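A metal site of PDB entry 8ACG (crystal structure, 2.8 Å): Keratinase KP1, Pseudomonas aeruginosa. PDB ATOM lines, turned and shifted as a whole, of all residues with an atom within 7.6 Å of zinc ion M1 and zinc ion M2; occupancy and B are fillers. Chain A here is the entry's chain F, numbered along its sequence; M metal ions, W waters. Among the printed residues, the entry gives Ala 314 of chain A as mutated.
The backbone NH of Glu 315 is in hydrogen-bond range of the side-chain carboxylate of Asp 272 (3.0 Å).
A ring nitrogen (NE2) of His 441 sits close to the side-chain hydroxyl (OH) of Tyr 440 (3.4 Å).
The side-chain amide nitrogen (ND2) of Asn 283 lies within hydrogen-bond range of the backbone carbonyl oxygen (O) of His 270.
A ring nitrogen (ND1) of His 270 lies within hydrogen-bond range of the backbone carbonyl oxygen of Asp 272, at 3.0 Å.
OD2 of Asp 343 sits at hydrogen-bond distance from OG of Ser 397, at 2.7 Å.
Zinc ion M1 is bound by a ring nitrogen (NE2) of His 441 (2.2 Å), the side-chain carboxylate of Asp 282 (2.3 Å) and the side-chain carboxylate of Glu 315 (2.3 Å).
Slightly farther from zinc ion M1 lies the side-chain carboxylate (OE1) of Glu 315 (2.6 Å).
OH of Tyr 440 touches zinc ion M1, 3.9 Å away.
Of the 22 residues printed, 4 come within 4 Å of zinc ion M1.
Zinc ion M2 is bound by OD1 of Asp 343.
Zinc ion M2 is bound by the side-chain carboxylate (OD1) of Asp 282 (2.1 Å).
A ring nitrogen (NE2) of His 270 binds zinc ion M2 (2.5 Å).
Zinc ion M2 has three donor atoms within binding distance.
Slightly farther from zinc ion M2 lies OD2 of Asp 343 (2.6 Å).
The nearest printed residue that does not touch zinc ion M2 is Met 344 (4.3 Å).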
ATOM      1  N   HIS A 270      -2.625  -2.070 -12.936  1.00  0.00           N
ATOM      2  CA  HIS A 270      -3.737  -2.164 -13.876  1.00  0.00           C
ATOM      3  C   HIS A 270      -4.365  -3.534 -13.741  1.00  0.00           C
ATOM      4  O   HIS A 270      -3.655  -4.542 -13.600  1.00  0.00           O
ATOM      5  CB  HIS A 270      -3.301  -1.897 -15.328  1.00  0.00           C
ATOM      6  CG  HIS A 270      -2.561  -3.017 -16.007  1.00  0.00           C
ATOM      7  ND1 HIS A 270      -3.198  -4.025 -16.699  1.00  0.00           N
ATOM      8  CD2 HIS A 270      -1.231  -3.249 -16.150  1.00  0.00           C
ATOM      9  CE1 HIS A 270      -2.305  -4.846 -17.207  1.00  0.00           C
ATOM     10  NE2 HIS A 270      -1.099  -4.395 -16.894  1.00  0.00           N
ATOM     11  N   ASP A 272      -6.940  -4.984 -15.770  1.00  0.00           N
ATOM     12  CA  ASP A 272      -7.387  -5.717 -16.949  1.00  0.00           C
ATOM     13  C   ASP A 272      -6.254  -6.547 -17.555  1.00  0.00           C
ATOM     14  O   ASP A 272      -5.067  -6.286 -17.320  1.00  0.00           O
ATOM     15  CB  ASP A 272      -7.908  -4.788 -18.015  1.00  0.00           C
ATOM     16  CG  ASP A 272      -6.815  -3.893 -18.563  1.00  0.00           C
ATOM     17  OD1 ASP A 272      -6.108  -3.309 -17.713  1.00  0.00           O
ATOM     18  OD2 ASP A 272      -6.639  -3.846 -19.811  1.00  0.00           O
ATOM     19  N   SER A 273      -6.643  -7.513 -18.372  1.00  0.00           N
ATOM     20  CA  SER A 273      -5.734  -8.341 -19.142  1.00  0.00           C
ATOM     21  C   SER A 273      -5.963  -8.129 -20.640  1.00  0.00           C
ATOM     22  O   SER A 273      -6.906  -7.455 -21.064  1.00  0.00           O
ATOM     23  CB  SER A 273      -5.924  -9.822 -18.815  1.00  0.00           C
ATOM     24  OG  SER A 273      -7.129 -10.325 -19.405  1.00  0.00           O
ATOM     25  N   VAL A 274      -5.086  -8.733 -21.443  1.00  0.00           N
ATOM     26  CA  VAL A 274      -5.317  -8.811 -22.877  1.00  0.00           C
ATOM     27  C   VAL A 274      -6.474  -9.771 -23.090  1.00  0.00           C
ATOM     28  O   VAL A 274      -6.907 -10.446 -22.151  1.00  0.00           O
ATOM     29  CB  VAL A 274      -4.074  -9.270 -23.673  1.00  0.00           C
ATOM     30  CG1 VAL A 274      -2.931  -8.322 -23.508  1.00  0.00           C
ATOM     31  CG2 VAL A 274      -3.697 -10.692 -23.272  1.00  0.00           C
ATOM     32  N   ASN A 281       0.073 -12.837 -14.480  1.00  0.00           N
ATOM     33  CA  ASN A 281       1.287 -12.059 -14.250  1.00  0.00           C
ATOM     34  C   ASN A 281       1.118 -10.642 -14.759  1.00  0.00           C
ATOM     35  O   ASN A 281       1.564  -9.680 -14.125  1.00  0.00           O
ATOM     36  CB  ASN A 281       2.465 -12.740 -14.949  1.00  0.00           C
ATOM     37  CG  ASN A 281       3.769 -12.059 -14.697  1.00  0.00           C
ATOM     38  OD1 ASN A 281       4.026 -11.570 -13.613  1.00  0.00           O
ATOM     39  ND2 ASN A 281       4.629 -12.059 -15.680  1.00  0.00           N
ATOM     40  N   ASP A 282       0.496 -10.479 -15.929  1.00  0.00           N
ATOM     41  CA  ASP A 282       0.277  -9.172 -16.520  1.00  0.00           C
ATOM     42  C   ASP A 282      -1.223  -8.916 -16.563  1.00  0.00           C
ATOM     43  O   ASP A 282      -1.887  -9.323 -17.518  1.00  0.00           O
ATOM     44  CB  ASP A 282       0.892  -9.094 -17.903  1.00  0.00           C
ATOM     45  CG  ASP A 282       0.727  -7.747 -18.538  1.00  0.00           C
ATOM     46  OD1 ASP A 282       0.620  -6.757 -17.787  1.00  0.00           O
ATOM     47  OD2 ASP A 282       0.669  -7.683 -19.784  1.00  0.00           O
ATOM     48  N   ASN A 283      -1.764  -8.251 -15.545  1.00  0.00           N
ATOM     49  CA  ASN A 283      -1.042  -7.761 -14.367  1.00  0.00           C
ATOM     50  C   ASN A 283      -1.788  -8.215 -13.120  1.00  0.00           C
ATOM     51  O   ASN A 283      -2.072  -7.417 -12.239  1.00  0.00           O
ATOM     52  CB  ASN A 283      -0.942  -6.234 -14.370  1.00  0.00           C
ATOM     53  CG  ASN A 283      -0.147  -5.687 -13.209  1.00  0.00           C
ATOM     54  OD1 ASN A 283       0.829  -6.273 -12.754  1.00  0.00           O
ATOM     55  ND2 ASN A 283      -0.597  -4.562 -12.688  1.00  0.00           N
ATOM     56  N   GLY A 284      -2.146  -9.500 -13.065  1.00  0.00           N
ATOM     57  CA  GLY A 284      -2.699 -10.009 -11.829  1.00  0.00           C
ATOM     58  C   GLY A 284      -1.730  -9.867 -10.680  1.00  0.00           C
ATOM     59  O   GLY A 284      -2.139  -9.608  -9.557  1.00  0.00           O
ATOM     60  N   ALA A 314      -6.014  -0.880 -19.449  1.00  0.00           N
ATOM     61  CA  ALA A 314      -4.633  -0.435 -19.667  1.00  0.00           C
ATOM     62  C   ALA A 314      -4.075  -1.072 -20.920  1.00  0.00           C
ATOM     63  O   ALA A 314      -3.309  -0.425 -21.640  1.00  0.00           O
ATOM     64  CB  ALA A 314      -3.741  -0.728 -18.470  1.00  0.00           C
ATOM     65  N   GLU A 315      -4.443  -2.335 -21.182  1.00  0.00           N
ATOM     66  CA  GLU A 315      -3.922  -2.989 -22.376  1.00  0.00           C
ATOM     67  C   GLU A 315      -4.449  -2.369 -23.642  1.00  0.00           C
ATOM     68  O   GLU A 315      -4.027  -2.768 -24.729  1.00  0.00           O
ATOM     69  CB  GLU A 315      -4.227  -4.502 -22.361  1.00  0.00           C
ATOM     70  CG  GLU A 315      -3.646  -5.217 -21.137  1.00  0.00           C
ATOM     71  CD  GLU A 315      -2.095  -5.364 -21.173  1.00  0.00           C
ATOM     72  OE1 GLU A 315      -1.452  -4.747 -22.035  1.00  0.00           O
ATOM     73  OE2 GLU A 315      -1.487  -6.022 -20.310  1.00  0.00           O
ATOM     74  N   LEU A 318      -3.407   2.531 -21.924  1.00  0.00           N
ATOM     75  CA  LEU A 318      -3.393   3.312 -20.688  1.00  0.00           C
ATOM     76  C   LEU A 318      -4.631   4.202 -20.542  1.00  0.00           C
ATOM     77  O   LEU A 318      -4.553   5.341 -20.066  1.00  0.00           O
ATOM     78  CB  LEU A 318      -2.112   4.148 -20.603  1.00  0.00           C
ATOM     79  CG  LEU A 318      -0.788   3.476 -20.956  1.00  0.00           C
ATOM     80  CD1 LEU A 318       0.371   4.432 -20.866  1.00  0.00           C
ATOM     81  CD2 LEU A 318      -0.540   2.286 -20.112  1.00  0.00           C
ATOM     82  N   ASN A 341       3.974   2.426  -9.373  1.00  0.00           N
ATOM     83  CA  ASN A 341       3.313   1.623 -10.380  1.00  0.00           C
ATOM     84  C   ASN A 341       3.872   0.225 -10.279  1.00  0.00           C
ATOM     85  O   ASN A 341       5.100   0.066 -10.230  1.00  0.00           O
ATOM     86  CB  ASN A 341       3.535   2.189 -11.794  1.00  0.00           C
ATOM     87  CG  ASN A 341       2.616   1.573 -12.815  1.00  0.00           C
ATOM     88  OD1 ASN A 341       1.411   1.809 -12.754  1.00  0.00           O
ATOM     89  ND2 ASN A 341       3.151   0.805 -13.757  1.00  0.00           N
ATOM     90  N   PHE A 342       2.994  -0.784 -10.215  1.00  0.00           N
ATOM     91  CA  PHE A 342       3.423  -2.171 -10.073  1.00  0.00           C
ATOM     92  C   PHE A 342       2.746  -3.004 -11.142  1.00  0.00           C
ATOM     93  O   PHE A 342       1.579  -3.356 -10.996  1.00  0.00           O
ATOM     94  CB  PHE A 342       3.150  -2.711  -8.681  1.00  0.00           C
ATOM     95  CG  PHE A 342       3.776  -1.872  -7.611  1.00  0.00           C
ATOM     96  CD1 PHE A 342       5.137  -1.939  -7.383  1.00  0.00           C
ATOM     97  CD2 PHE A 342       3.020  -0.993  -6.862  1.00  0.00           C
ATOM     98  CE1 PHE A 342       5.713  -1.167  -6.455  1.00  0.00           C
ATOM     99  CE2 PHE A 342       3.617  -0.212  -5.917  1.00  0.00           C
ATOM    100  CZ  PHE A 342       4.969  -0.310  -5.722  1.00  0.00           C
ATOM    101  N   ASP A 343       3.497  -3.291 -12.215  1.00  0.00           N
ATOM    102  CA  ASP A 343       2.985  -3.910 -13.434  1.00  0.00           C
ATOM    103  C   ASP A 343       3.913  -5.061 -13.827  1.00  0.00           C
ATOM    104  O   ASP A 343       5.008  -4.817 -14.333  1.00  0.00           O
ATOM    105  CB  ASP A 343       2.923  -2.884 -14.551  1.00  0.00           C
ATOM    106  CG  ASP A 343       2.213  -3.370 -15.782  1.00  0.00           C
ATOM    107  OD1 ASP A 343       2.106  -4.597 -16.000  1.00  0.00           O
ATOM    108  OD2 ASP A 343       1.748  -2.513 -16.562  1.00  0.00           O
ATOM    109  N   MET A 344       3.438  -6.302 -13.644  1.00  0.00           N
ATOM    110  CA  MET A 344       4.194  -7.524 -13.908  1.00  0.00           C
ATOM    111  C   MET A 344       5.336  -7.722 -12.930  1.00  0.00           C
ATOM    112  O   MET A 344       6.465  -7.320 -13.213  1.00  0.00           O
ATOM    113  CB  MET A 344       4.764  -7.553 -15.320  1.00  0.00           C
ATOM    114  CG  MET A 344       3.777  -7.852 -16.381  1.00  0.00           C
ATOM    115  SD  MET A 344       4.570  -7.873 -17.988  1.00  0.00           S
ATOM    116  CE  MET A 344       5.390  -9.464 -17.958  1.00  0.00           C
ATOM    117  N   ARG A 396       5.465   3.446 -20.825  1.00  0.00           N
ATOM    118  CA  ARG A 396       5.073   2.108 -21.235  1.00  0.00           C
ATOM    119  C   ARG A 396       3.941   1.525 -20.381  1.00  0.00           C
ATOM    120  O   ARG A 396       3.350   0.497 -20.767  1.00  0.00           O
ATOM    121  CB  ARG A 396       6.290   1.201 -21.111  1.00  0.00           C
ATOM    122  CG  ARG A 396       7.585   1.717 -21.711  1.00  0.00           C
ATOM    123  CD  ARG A 396       8.711   0.653 -21.454  1.00  0.00           C
ATOM    124  NE  ARG A 396      10.028   0.963 -22.029  1.00  0.00           N
ATOM    125  CZ  ARG A 396      10.484   0.438 -23.174  1.00  0.00           C
ATOM    126  NH1 ARG A 396      11.699   0.762 -23.648  1.00  0.00           N
ATOM    127  NH2 ARG A 396       9.724  -0.386 -23.882  1.00  0.00           N
ATOM    128  N   SER A 397       3.634   2.155 -19.243  1.00  0.00           N
ATOM    129  CA  SER A 397       2.649   1.623 -18.303  1.00  0.00           C
ATOM    130  C   SER A 397       1.919   2.813 -17.674  1.00  0.00           C
ATOM    131  O   SER A 397       2.106   3.953 -18.076  1.00  0.00           O
ATOM    132  CB  SER A 397       3.363   0.756 -17.265  1.00  0.00           C
ATOM    133  OG  SER A 397       2.422   0.107 -16.450  1.00  0.00           O
ATOM    134  N   ASP A 398       1.090   2.536 -16.662  1.00  0.00           N
ATOM    135  CA  ASP A 398       0.096   3.488 -16.170  1.00  0.00           C
ATOM    136  C   ASP A 398       0.656   4.664 -15.398  1.00  0.00           C
ATOM    137  O   ASP A 398      -0.134   5.484 -14.963  1.00  0.00           O
ATOM    138  CB  ASP A 398      -0.939   2.787 -15.303  1.00  0.00           C
ATOM    139  CG  ASP A 398      -1.725   1.795 -16.079  1.00  0.00           C
ATOM    140  OD1 ASP A 398      -2.563   2.236 -16.915  1.00  0.00           O
ATOM    141  OD2 ASP A 398      -1.496   0.583 -15.909  1.00  0.00           O
ATOM    142  N   PHE A 413       9.273  -3.951 -11.957  1.00  0.00           N
ATOM    143  CA  PHE A 413       9.069  -4.686 -13.194  1.00  0.00           C
ATOM    144  C   PHE A 413       9.950  -5.910 -13.092  1.00  0.00           C
ATOM    145  O   PHE A 413      11.076  -5.811 -12.577  1.00  0.00           O
ATOM    146  CB  PHE A 413       9.463  -3.858 -14.413  1.00  0.00           C
ATOM    147  CG  PHE A 413       9.150  -4.513 -15.736  1.00  0.00           C
ATOM    148  CD1 PHE A 413       7.954  -5.174 -15.931  1.00  0.00           C
ATOM    149  CD2 PHE A 413      10.025  -4.402 -16.801  1.00  0.00           C
ATOM    150  CE1 PHE A 413       7.654  -5.752 -17.166  1.00  0.00           C
ATOM    151  CE2 PHE A 413       9.720  -4.949 -18.023  1.00  0.00           C
ATOM    152  CZ  PHE A 413       8.536  -5.628 -18.211  1.00  0.00           C
ATOM    153  N   ALA A 416       9.442  -8.635 -19.464  1.00  0.00           N
ATOM    154  CA  ALA A 416       8.403  -9.181 -20.332  1.00  0.00           C
ATOM    155  C   ALA A 416       8.975  -9.923 -21.519  1.00  0.00           C
ATOM    156  O   ALA A 416       9.433 -11.054 -21.374  1.00  0.00           O
ATOM    157  CB  ALA A 416       7.441  -8.093 -20.803  1.00  0.00           C
ATOM    158  N   TYR A 440       4.036 -14.021 -22.035  1.00  0.00           N
ATOM    159  CA  TYR A 440       3.592 -12.626 -22.089  1.00  0.00           C
ATOM    160  C   TYR A 440       2.469 -12.412 -23.102  1.00  0.00           C
ATOM    161  O   TYR A 440       2.574 -12.780 -24.271  1.00  0.00           O
ATOM    162  CB  TYR A 440       4.794 -11.757 -22.447  1.00  0.00           C
ATOM    163  CG  TYR A 440       4.486 -10.311 -22.694  1.00  0.00           C
ATOM    164  CD1 TYR A 440       3.967  -9.501 -21.700  1.00  0.00           C
ATOM    165  CD2 TYR A 440       4.770  -9.751 -23.927  1.00  0.00           C
ATOM    166  CE1 TYR A 440       3.714  -8.170 -21.929  1.00  0.00           C
ATOM    167  CE2 TYR A 440       4.525  -8.428 -24.175  1.00  0.00           C
ATOM    168  CZ  TYR A 440       3.986  -7.632 -23.183  1.00  0.00           C
ATOM    169  OH  TYR A 440       3.737  -6.296 -23.433  1.00  0.00           O
ATOM    170  N   HIS A 441       1.385 -11.831 -22.603  1.00  0.00           N
ATOM    171  CA  HIS A 441       0.205 -11.518 -23.389  1.00  0.00           C
ATOM    172  C   HIS A 441      -0.366 -12.757 -24.062  1.00  0.00           C
ATOM    173  O   HIS A 441      -1.054 -12.657 -25.073  1.00  0.00           O
ATOM    174  CB  HIS A 441       0.472 -10.420 -24.409  1.00  0.00           C
ATOM    175  CG  HIS A 441       0.567  -9.067 -23.793  1.00  0.00           C
ATOM    176  ND1 HIS A 441       0.766  -7.917 -24.535  1.00  0.00           N
ATOM    177  CD2 HIS A 441       0.489  -8.673 -22.503  1.00  0.00           C
ATOM    178  CE1 HIS A 441       0.786  -6.871 -23.723  1.00  0.00           C
ATOM    179  NE2 HIS A 441       0.632  -7.301 -22.486  1.00  0.00           N
HETATM  180 ZN    ZN M   1       0.720  -5.732 -20.951  1.00  0.00          ZN
HETATM  181 ZN    ZN M   2       1.173  -4.721 -17.867  1.00  0.00          ZN
HETATM  182  O   HOH W   1       3.516  -5.126 -19.964  1.00  0.00           O
